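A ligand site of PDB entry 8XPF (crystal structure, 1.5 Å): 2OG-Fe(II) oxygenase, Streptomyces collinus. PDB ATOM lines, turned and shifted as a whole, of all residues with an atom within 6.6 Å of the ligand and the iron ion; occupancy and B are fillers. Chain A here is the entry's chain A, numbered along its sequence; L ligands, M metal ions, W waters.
Water W4 lies within hydrogen-bond range of the backbone carbonyl oxygen (O) of Gly 136 (3.0 Å) and an oxygen (O2) of the ligand (3.4 Å).
OH of Tyr 135 sits close to O of Asp 115 (3.4 Å). The side-chain hydroxyl (OG1) of Thr 150 sits at hydrogen-bond distance from the side-chain hydroxyl (OH) of Tyr 139. O of Lys 99 sits at hydrogen-bond distance from N of Arg 215 (2.8 Å). The guanidinium group (NH1) of Arg 215 sits at hydrogen-bond distance from the backbone carbonyl oxygen (O) of Ala 148, at 2.9 Å. The side-chain amide oxygen (OE1) of Gln 110 is in hydrogen-bond range of the backbone NH (N) of Gly 205 (2.9 Å). The backbone NH (N) of Tyr 135 sits at hydrogen-bond distance from the backbone carbonyl oxygen (O) of Phe 197. The backbone NH (N) of Ile 137 sits at hydrogen-bond distance from the backbone carbonyl oxygen (O) of Leu 195. The backbone NH (N) of Phe 219 lies within hydrogen-bond range of the backbone carbonyl oxygen (O) of Phe 95 (2.8 Å).
Three residues have an atom within 4 Å of the iron ion: His 113, Asp 115 and His 203.
The iron ion is bound by the side-chain carboxylate (OD2) of Asp 115 (2.0 Å), water W2 (2.1 Å), an oxygen (O3) of the ligand (2.1 Å), a ring nitrogen (NE2) of His 203 (2.2 Å), a ring nitrogen (NE2) of His 113 (2.2 Å) and an oxygen (O1) of the ligand (2.2 Å). The iron ion has six donor atoms within binding distance.
Ile 137 touches the ligand. CZ of Phe 197 touches O1 of the ligand, 3.6 Å away. Gly 205 touches the ligand. CD2 of Phe 219 touches O2 of the ligand, at 3.7 Å. Of the 23 residues printed, 10 come within 4 Å of the ligand. The nearest printed residue that does not touch the ligand is Tyr 135 (4.03 Å).
OG1 of Thr 150 sits at hydrogen-bond distance from O5 of the ligand (2.6 Å). O4 of the ligand is in salt-bridge range of NH2 of Arg 215, 2.7 Å away. An oxygen (O3) of the ligand lies close to the side-chain amide oxygen (OE1) of Gln 110 (3.3 Å).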
ATOM      1  N   PHE A  95      25.080  19.046  15.204  1.00  0.00           N
ATOM      2  CA  PHE A  95      25.235  19.622  16.530  1.00  0.00           C
ATOM      3  C   PHE A  95      24.502  18.744  17.527  1.00  0.00           C
ATOM      4  O   PHE A  95      23.678  17.905  17.141  1.00  0.00           O
ATOM      5  CB  PHE A  95      24.721  21.081  16.600  1.00  0.00           C
ATOM      6  CG  PHE A  95      23.262  21.231  16.245  1.00  0.00           C
ATOM      7  CD1 PHE A  95      22.300  21.168  17.244  1.00  0.00           C
ATOM      8  CD2 PHE A  95      22.858  21.470  14.941  1.00  0.00           C
ATOM      9  CE1 PHE A  95      20.940  21.332  16.935  1.00  0.00           C
ATOM     10  CE2 PHE A  95      21.495  21.614  14.620  1.00  0.00           C
ATOM     11  CZ  PHE A  95      20.559  21.547  15.634  1.00  0.00           C
ATOM     12  N   GLN A  97      22.234  19.028  21.259  1.00  0.00           N
ATOM     13  CA  GLN A  97      21.519  20.011  22.053  1.00  0.00           C
ATOM     14  C   GLN A  97      20.689  19.314  23.112  1.00  0.00           C
ATOM     15  O   GLN A  97      20.182  18.201  22.905  1.00  0.00           O
ATOM     16  CB  GLN A  97      20.606  20.891  21.180  1.00  0.00           C
ATOM     17  CG  GLN A  97      20.109  22.168  21.884  1.00  0.00           C
ATOM     18  CD  GLN A  97      19.372  23.104  20.942  1.00  0.00           C
ATOM     19  OE1 GLN A  97      18.583  22.675  20.085  1.00  0.00           O
ATOM     20  NE2 GLN A  97      19.596  24.414  21.121  1.00  0.00           N
ATOM     21  N   LYS A  99      17.331  20.109  25.633  1.00  0.00           N
ATOM     22  CA  LYS A  99      16.197  20.987  25.866  1.00  0.00           C
ATOM     23  C   LYS A  99      15.661  20.698  27.264  1.00  0.00           C
ATOM     24  O   LYS A  99      15.226  19.578  27.544  1.00  0.00           O
ATOM     25  CB  LYS A  99      15.097  20.771  24.826  1.00  0.00           C
ATOM     26  CG  LYS A  99      14.007  21.801  24.923  1.00  0.00           C
ATOM     27  CD  LYS A  99      13.002  21.649  23.815  1.00  0.00           C
ATOM     28  CE  LYS A  99      13.528  22.182  22.511  1.00  0.00           C
ATOM     29  NZ  LYS A  99      12.406  22.371  21.530  1.00  0.00           N
ATOM     30  N   GLN A 110       8.555  26.569  19.063  1.00  0.00           N
ATOM     31  CA  GLN A 110       8.915  27.217  17.813  1.00  0.00           C
ATOM     32  C   GLN A 110       7.664  27.359  16.945  1.00  0.00           C
ATOM     33  O   GLN A 110       6.692  26.619  17.089  1.00  0.00           O
ATOM     34  CB  GLN A 110       9.893  26.342  17.032  1.00  0.00           C
ATOM     35  CG  GLN A 110      11.276  26.166  17.627  1.00  0.00           C
ATOM     36  CD  GLN A 110      12.209  25.349  16.714  1.00  0.00           C
ATOM     37  OE1 GLN A 110      11.763  24.547  15.896  1.00  0.00           O
ATOM     38  NE2 GLN A 110      13.510  25.560  16.872  1.00  0.00           N
ATOM     39  N   HIS A 113       7.666  25.687  10.474  1.00  0.00           N
ATOM     40  CA  HIS A 113       8.565  26.247   9.464  1.00  0.00           C
ATOM     41  C   HIS A 113       9.047  25.113   8.569  1.00  0.00           C
ATOM     42  O   HIS A 113       8.853  23.930   8.865  1.00  0.00           O
ATOM     43  CB  HIS A 113       9.768  26.925  10.136  1.00  0.00           C
ATOM     44  CG  HIS A 113      10.639  25.985  10.912  1.00  0.00           C
ATOM     45  ND1 HIS A 113      10.383  25.667  12.234  1.00  0.00           N
ATOM     46  CD2 HIS A 113      11.740  25.286  10.557  1.00  0.00           C
ATOM     47  CE1 HIS A 113      11.306  24.820  12.659  1.00  0.00           C
ATOM     48  NE2 HIS A 113      12.128  24.560  11.659  1.00  0.00           N
ATOM     49  N   ASN A 114       9.669  25.496   7.455  1.00  0.00           N
ATOM     50  CA  ASN A 114      10.450  24.563   6.664  1.00  0.00           C
ATOM     51  C   ASN A 114      11.933  24.886   6.827  1.00  0.00           C
ATOM     52  O   ASN A 114      12.312  25.979   7.244  1.00  0.00           O
ATOM     53  CB  ASN A 114      10.055  24.581   5.167  1.00  0.00           C
ATOM     54  CG  ASN A 114      10.517  25.844   4.442  1.00  0.00           C
ATOM     55  OD1 ASN A 114      11.706  26.022   4.172  1.00  0.00           O
ATOM     56  ND2 ASN A 114       9.581  26.726   4.121  1.00  0.00           N
ATOM     57  N   ASP A 115      12.745  23.873   6.544  1.00  0.00           N
ATOM     58  CA  ASP A 115      14.201  24.052   6.529  1.00  0.00           C
ATOM     59  C   ASP A 115      14.703  23.717   5.140  1.00  0.00           C
ATOM     60  O   ASP A 115      15.644  22.936   4.956  1.00  0.00           O
ATOM     61  CB  ASP A 115      14.867  23.163   7.588  1.00  0.00           C
ATOM     62  CG  ASP A 115      14.708  23.697   8.987  1.00  0.00           C
ATOM     63  OD1 ASP A 115      15.245  24.796   9.280  1.00  0.00           O
ATOM     64  OD2 ASP A 115      14.035  23.044   9.803  1.00  0.00           O
ATOM     65  N   TYR A 135      17.245  15.909   6.967  1.00  0.00           N
ATOM     66  CA  TYR A 135      17.546  16.190   8.369  1.00  0.00           C
ATOM     67  C   TYR A 135      17.408  14.924   9.188  1.00  0.00           C
ATOM     68  O   TYR A 135      16.545  14.084   8.911  1.00  0.00           O
ATOM     69  CB  TYR A 135      16.560  17.234   8.935  1.00  0.00           C
ATOM     70  CG  TYR A 135      16.927  18.627   8.506  1.00  0.00           C
ATOM     71  CD1 TYR A 135      16.770  19.027   7.189  1.00  0.00           C
ATOM     72  CD2 TYR A 135      17.464  19.525   9.419  1.00  0.00           C
ATOM     73  CE1 TYR A 135      17.141  20.298   6.786  1.00  0.00           C
ATOM     74  CE2 TYR A 135      17.826  20.796   9.026  1.00  0.00           C
ATOM     75  CZ  TYR A 135      17.660  21.168   7.711  1.00  0.00           C
ATOM     76  OH  TYR A 135      18.041  22.432   7.357  1.00  0.00           O
ATOM     77  N   GLY A 136      18.255  14.786  10.189  1.00  0.00           N
ATOM     78  CA  GLY A 136      18.109  13.704  11.153  1.00  0.00           C
ATOM     79  C   GLY A 136      18.136  14.249  12.573  1.00  0.00           C
ATOM     80  O   GLY A 136      18.884  15.178  12.876  1.00  0.00           O
ATOM     81  N   ILE A 137      17.338  13.640  13.436  1.00  0.00           N
ATOM     82  CA  ILE A 137      17.418  13.859  14.872  1.00  0.00           C
ATOM     83  C   ILE A 137      17.523  12.493  15.515  1.00  0.00           C
ATOM     84  O   ILE A 137      16.606  11.682  15.420  1.00  0.00           O
ATOM     85  CB  ILE A 137      16.199  14.607  15.417  1.00  0.00           C
ATOM     86  CG1 ILE A 137      15.966  15.890  14.627  1.00  0.00           C
ATOM     87  CG2 ILE A 137      16.423  14.929  16.882  1.00  0.00           C
ATOM     88  CD1 ILE A 137      14.735  16.684  15.082  1.00  0.00           C
ATOM     89  N   TYR A 139      17.521  10.711  18.861  1.00  0.00           N
ATOM     90  CA  TYR A 139      17.116  10.998  20.226  1.00  0.00           C
ATOM     91  C   TYR A 139      17.889  10.106  21.172  1.00  0.00           C
ATOM     92  O   TYR A 139      17.924   8.885  20.994  1.00  0.00           O
ATOM     93  CB  TYR A 139      15.618  10.736  20.389  1.00  0.00           C
ATOM     94  CG  TYR A 139      14.764  11.566  19.455  1.00  0.00           C
ATOM     95  CD1 TYR A 139      14.547  12.914  19.702  1.00  0.00           C
ATOM     96  CD2 TYR A 139      14.180  10.996  18.337  1.00  0.00           C
ATOM     97  CE1 TYR A 139      13.742  13.685  18.846  1.00  0.00           C
ATOM     98  CE2 TYR A 139      13.374  11.747  17.490  1.00  0.00           C
ATOM     99  CZ  TYR A 139      13.176  13.079  17.735  1.00  0.00           C
ATOM    100  OH  TYR A 139      12.358  13.805  16.876  1.00  0.00           O
ATOM    101  N   ALA A 148       9.179  17.577  25.011  1.00  0.00           N
ATOM    102  CA  ALA A 148       9.512  18.406  23.849  1.00  0.00           C
ATOM    103  C   ALA A 148       9.626  17.593  22.559  1.00  0.00           C
ATOM    104  O   ALA A 148      10.662  17.641  21.884  1.00  0.00           O
ATOM    105  CB  ALA A 148      10.800  19.204  24.091  1.00  0.00           C
ATOM    106  N   PRO A 149       8.581  16.875  22.175  1.00  0.00           N
ATOM    107  CA  PRO A 149       8.634  16.131  20.913  1.00  0.00           C
ATOM    108  C   PRO A 149       8.704  17.064  19.714  1.00  0.00           C
ATOM    109  O   PRO A 149       8.193  18.191  19.744  1.00  0.00           O
ATOM    110  CB  PRO A 149       7.310  15.364  20.909  1.00  0.00           C
ATOM    111  CG  PRO A 149       6.394  16.232  21.710  1.00  0.00           C
ATOM    112  CD  PRO A 149       7.270  16.743  22.824  1.00  0.00           C
ATOM    113  N   THR A 150       9.353  16.584  18.662  1.00  0.00           N
ATOM    114  CA  THR A 150       9.247  17.213  17.350  1.00  0.00           C
ATOM    115  C   THR A 150       7.816  17.081  16.832  1.00  0.00           C
ATOM    116  O   THR A 150       7.187  16.031  16.987  1.00  0.00           O
ATOM    117  CB  THR A 150      10.170  16.497  16.377  1.00  0.00           C
ATOM    118  OG1 THR A 150      11.492  16.417  16.932  1.00  0.00           O
ATOM    119  CG2 THR A 150      10.260  17.255  15.064  1.00  0.00           C
ATOM    120  N   TYR A 151       7.288  18.152  16.243  1.00  0.00           N
ATOM    121  CA  TYR A 151       5.993  18.106  15.561  1.00  0.00           C
ATOM    122  C   TYR A 151       6.208  18.145  14.058  1.00  0.00           C
ATOM    123  O   TYR A 151       7.085  18.862  13.561  1.00  0.00           O
ATOM    124  CB  TYR A 151       5.095  19.273  15.964  1.00  0.00           C
ATOM    125  CG  TYR A 151       4.328  19.093  17.257  1.00  0.00           C
ATOM    126  CD1 TYR A 151       4.984  19.172  18.484  1.00  0.00           C
ATOM    127  CD2 TYR A 151       2.963  18.848  17.244  1.00  0.00           C
ATOM    128  CE1 TYR A 151       4.292  19.014  19.672  1.00  0.00           C
ATOM    129  CE2 TYR A 151       2.272  18.686  18.424  1.00  0.00           C
ATOM    130  CZ  TYR A 151       2.944  18.773  19.625  1.00  0.00           C
ATOM    131  OH  TYR A 151       2.226  18.614  20.790  1.00  0.00           O
ATOM    132  N   LEU A 195      14.776  10.174  13.819  1.00  0.00           N
ATOM    133  CA  LEU A 195      13.785  10.792  12.954  1.00  0.00           C
ATOM    134  C   LEU A 195      14.519  11.362  11.748  1.00  0.00           C
ATOM    135  O   LEU A 195      15.445  12.174  11.910  1.00  0.00           O
ATOM    136  CB  LEU A 195      13.020  11.907  13.670  1.00  0.00           C
ATOM    137  CG  LEU A 195      12.015  12.647  12.790  1.00  0.00           C
ATOM    138  CD1 LEU A 195      10.875  11.724  12.397  1.00  0.00           C
ATOM    139  CD2 LEU A 195      11.482  13.891  13.518  1.00  0.00           C
ATOM    140  N   PHE A 197      13.805  13.514   8.144  1.00  0.00           N
ATOM    141  CA  PHE A 197      12.794  14.304   7.462  1.00  0.00           C
ATOM    142  C   PHE A 197      13.411  15.133   6.346  1.00  0.00           C
ATOM    143  O   PHE A 197      14.605  15.433   6.352  1.00  0.00           O
ATOM    144  CB  PHE A 197      11.933  15.147   8.423  1.00  0.00           C
ATOM    145  CG  PHE A 197      12.681  16.200   9.201  1.00  0.00           C
ATOM    146  CD1 PHE A 197      12.807  17.495   8.711  1.00  0.00           C
ATOM    147  CD2 PHE A 197      13.163  15.923  10.473  1.00  0.00           C
ATOM    148  CE1 PHE A 197      13.440  18.471   9.460  1.00  0.00           C
ATOM    149  CE2 PHE A 197      13.810  16.892  11.216  1.00  0.00           C
ATOM    150  CZ  PHE A 197      13.923  18.166  10.724  1.00  0.00           C
ATOM    151  N   HIS A 203       7.292  21.645  10.039  1.00  0.00           N
ATOM    152  CA  HIS A 203       7.573  20.979  11.293  1.00  0.00           C
ATOM    153  C   HIS A 203       7.993  22.042  12.306  1.00  0.00           C
ATOM    154  O   HIS A 203       8.223  23.203  11.956  1.00  0.00           O
ATOM    155  CB  HIS A 203       8.713  19.963  11.127  1.00  0.00           C
ATOM    156  CG  HIS A 203      10.023  20.624  10.846  1.00  0.00           C
ATOM    157  ND1 HIS A 203      10.375  21.096   9.602  1.00  0.00           N
ATOM    158  CD2 HIS A 203      11.052  20.953  11.671  1.00  0.00           C
ATOM    159  CE1 HIS A 203      11.567  21.659   9.660  1.00  0.00           C
ATOM    160  NE2 HIS A 203      11.990  21.602  10.911  1.00  0.00           N
ATOM    161  N   ARG A 204       8.156  21.612  13.560  1.00  0.00           N
ATOM    162  CA  ARG A 204       8.671  22.517  14.579  1.00  0.00           C
ATOM    163  C   ARG A 204       9.165  21.704  15.765  1.00  0.00           C
ATOM    164  O   ARG A 204       8.739  20.571  15.986  1.00  0.00           O
ATOM    165  CB  ARG A 204       7.603  23.497  15.057  1.00  0.00           C
ATOM    166  CG  ARG A 204       6.446  22.838  15.805  1.00  0.00           C
ATOM    167  CD  ARG A 204       5.436  23.883  16.279  1.00  0.00           C
ATOM    168  NE  ARG A 204       4.296  23.292  16.973  1.00  0.00           N
ATOM    169  CZ  ARG A 204       4.258  23.098  18.287  1.00  0.00           C
ATOM    170  NH1 ARG A 204       5.278  23.433  19.063  1.00  0.00           N
ATOM    171  NH2 ARG A 204       3.174  22.556  18.828  1.00  0.00           N
ATOM    172  N   GLY A 205      10.061  22.312  16.545  1.00  0.00           N
ATOM    173  CA  GLY A 205      10.259  21.885  17.912  1.00  0.00           C
ATOM    174  C   GLY A 205       9.146  22.389  18.815  1.00  0.00           C
ATOM    175  O   GLY A 205       8.335  23.251  18.448  1.00  0.00           O
ATOM    176  N   SER A 206       9.085  21.825  20.016  1.00  0.00           N
ATOM    177  CA  SER A 206       8.013  22.151  20.942  1.00  0.00           C
ATOM    178  C   SER A 206       8.561  22.397  22.335  1.00  0.00           C
ATOM    179  O   SER A 206       9.702  22.084  22.654  1.00  0.00           O
ATOM    180  CB  SER A 206       6.910  21.076  20.959  1.00  0.00           C
ATOM    181  OG  SER A 206       7.370  19.875  21.583  1.00  0.00           O
ATOM    182  N   ARG A 215      15.642  16.811  27.338  1.00  0.00           N
ATOM    183  CA  ARG A 215      15.731  15.984  26.141  1.00  0.00           C
ATOM    184  C   ARG A 215      17.135  16.107  25.571  1.00  0.00           C
ATOM    185  O   ARG A 215      17.666  17.215  25.459  1.00  0.00           O
ATOM    186  CB  ARG A 215      14.719  16.441  25.085  1.00  0.00           C
ATOM    187  CG  ARG A 215      14.634  15.490  23.900  1.00  0.00           C
ATOM    188  CD  ARG A 215      13.795  16.048  22.742  1.00  0.00           C
ATOM    189  NE  ARG A 215      14.526  17.055  21.994  1.00  0.00           N
ATOM    190  CZ  ARG A 215      14.132  17.560  20.830  1.00  0.00           C
ATOM    191  NH1 ARG A 215      13.004  17.164  20.264  1.00  0.00           N
ATOM    192  NH2 ARG A 215      14.890  18.457  20.226  1.00  0.00           N
ATOM    193  N   PHE A 219      21.749  16.181  16.181  1.00  0.00           N
ATOM    194  CA  PHE A 219      21.097  16.683  14.988  1.00  0.00           C
ATOM    195  C   PHE A 219      22.110  16.689  13.853  1.00  0.00           C
ATOM    196  O   PHE A 219      23.293  16.914  14.084  1.00  0.00           O
ATOM    197  CB  PHE A 219      20.672  18.134  15.191  1.00  0.00           C
ATOM    198  CG  PHE A 219      19.628  18.317  16.244  1.00  0.00           C
ATOM    199  CD1 PHE A 219      19.969  18.225  17.583  1.00  0.00           C
ATOM    200  CD2 PHE A 219      18.332  18.644  15.895  1.00  0.00           C
ATOM    201  CE1 PHE A 219      19.010  18.419  18.570  1.00  0.00           C
ATOM    202  CE2 PHE A 219      17.369  18.841  16.869  1.00  0.00           C
ATOM    203  CZ  PHE A 219      17.714  18.741  18.212  1.00  0.00           C
HETATM  204  C1  LIG L   1      14.881  20.903  13.200  1.00  0.00           C
HETATM  205  O1  LIG L   1      14.977  21.306  12.036  1.00  0.00           O
HETATM  206  O2  LIG L   1      15.620  19.931  13.715  1.00  0.00           O
HETATM  207  C2  LIG L   1      13.877  21.558  14.185  1.00  0.00           C
HETATM  208  O3  LIG L   1      13.076  22.373  13.741  1.00  0.00           O
HETATM  209  C3  LIG L   1      13.964  21.210  15.649  1.00  0.00           C
HETATM  210  C4  LIG L   1      12.971  20.143  16.072  1.00  0.00           C
HETATM  211  C5  LIG L   1      13.212  19.635  17.480  1.00  0.00           C
HETATM  212  O4  LIG L   1      14.072  20.087  18.211  1.00  0.00           O
HETATM  213  O5  LIG L   1      12.415  18.674  17.834  1.00  0.00           O
HETATM  214 FE    FE M   1      13.519  22.890  11.704  1.00  0.00          FE
HETATM  215  O   HOH W   1      18.183  21.887  12.445  1.00  0.00           O
HETATM  216  O   HOH W   2      15.101  24.153  12.324  1.00  0.00           O
HETATM  217  O   HOH W   3      17.074  22.573  15.075  1.00  0.00           O
HETATM  218  O   HOH W   4      18.023  17.971  12.367  1.00  0.00           O
HETATM  219  O   HOH W   5      11.315  19.933  20.334  1.00  0.00           O
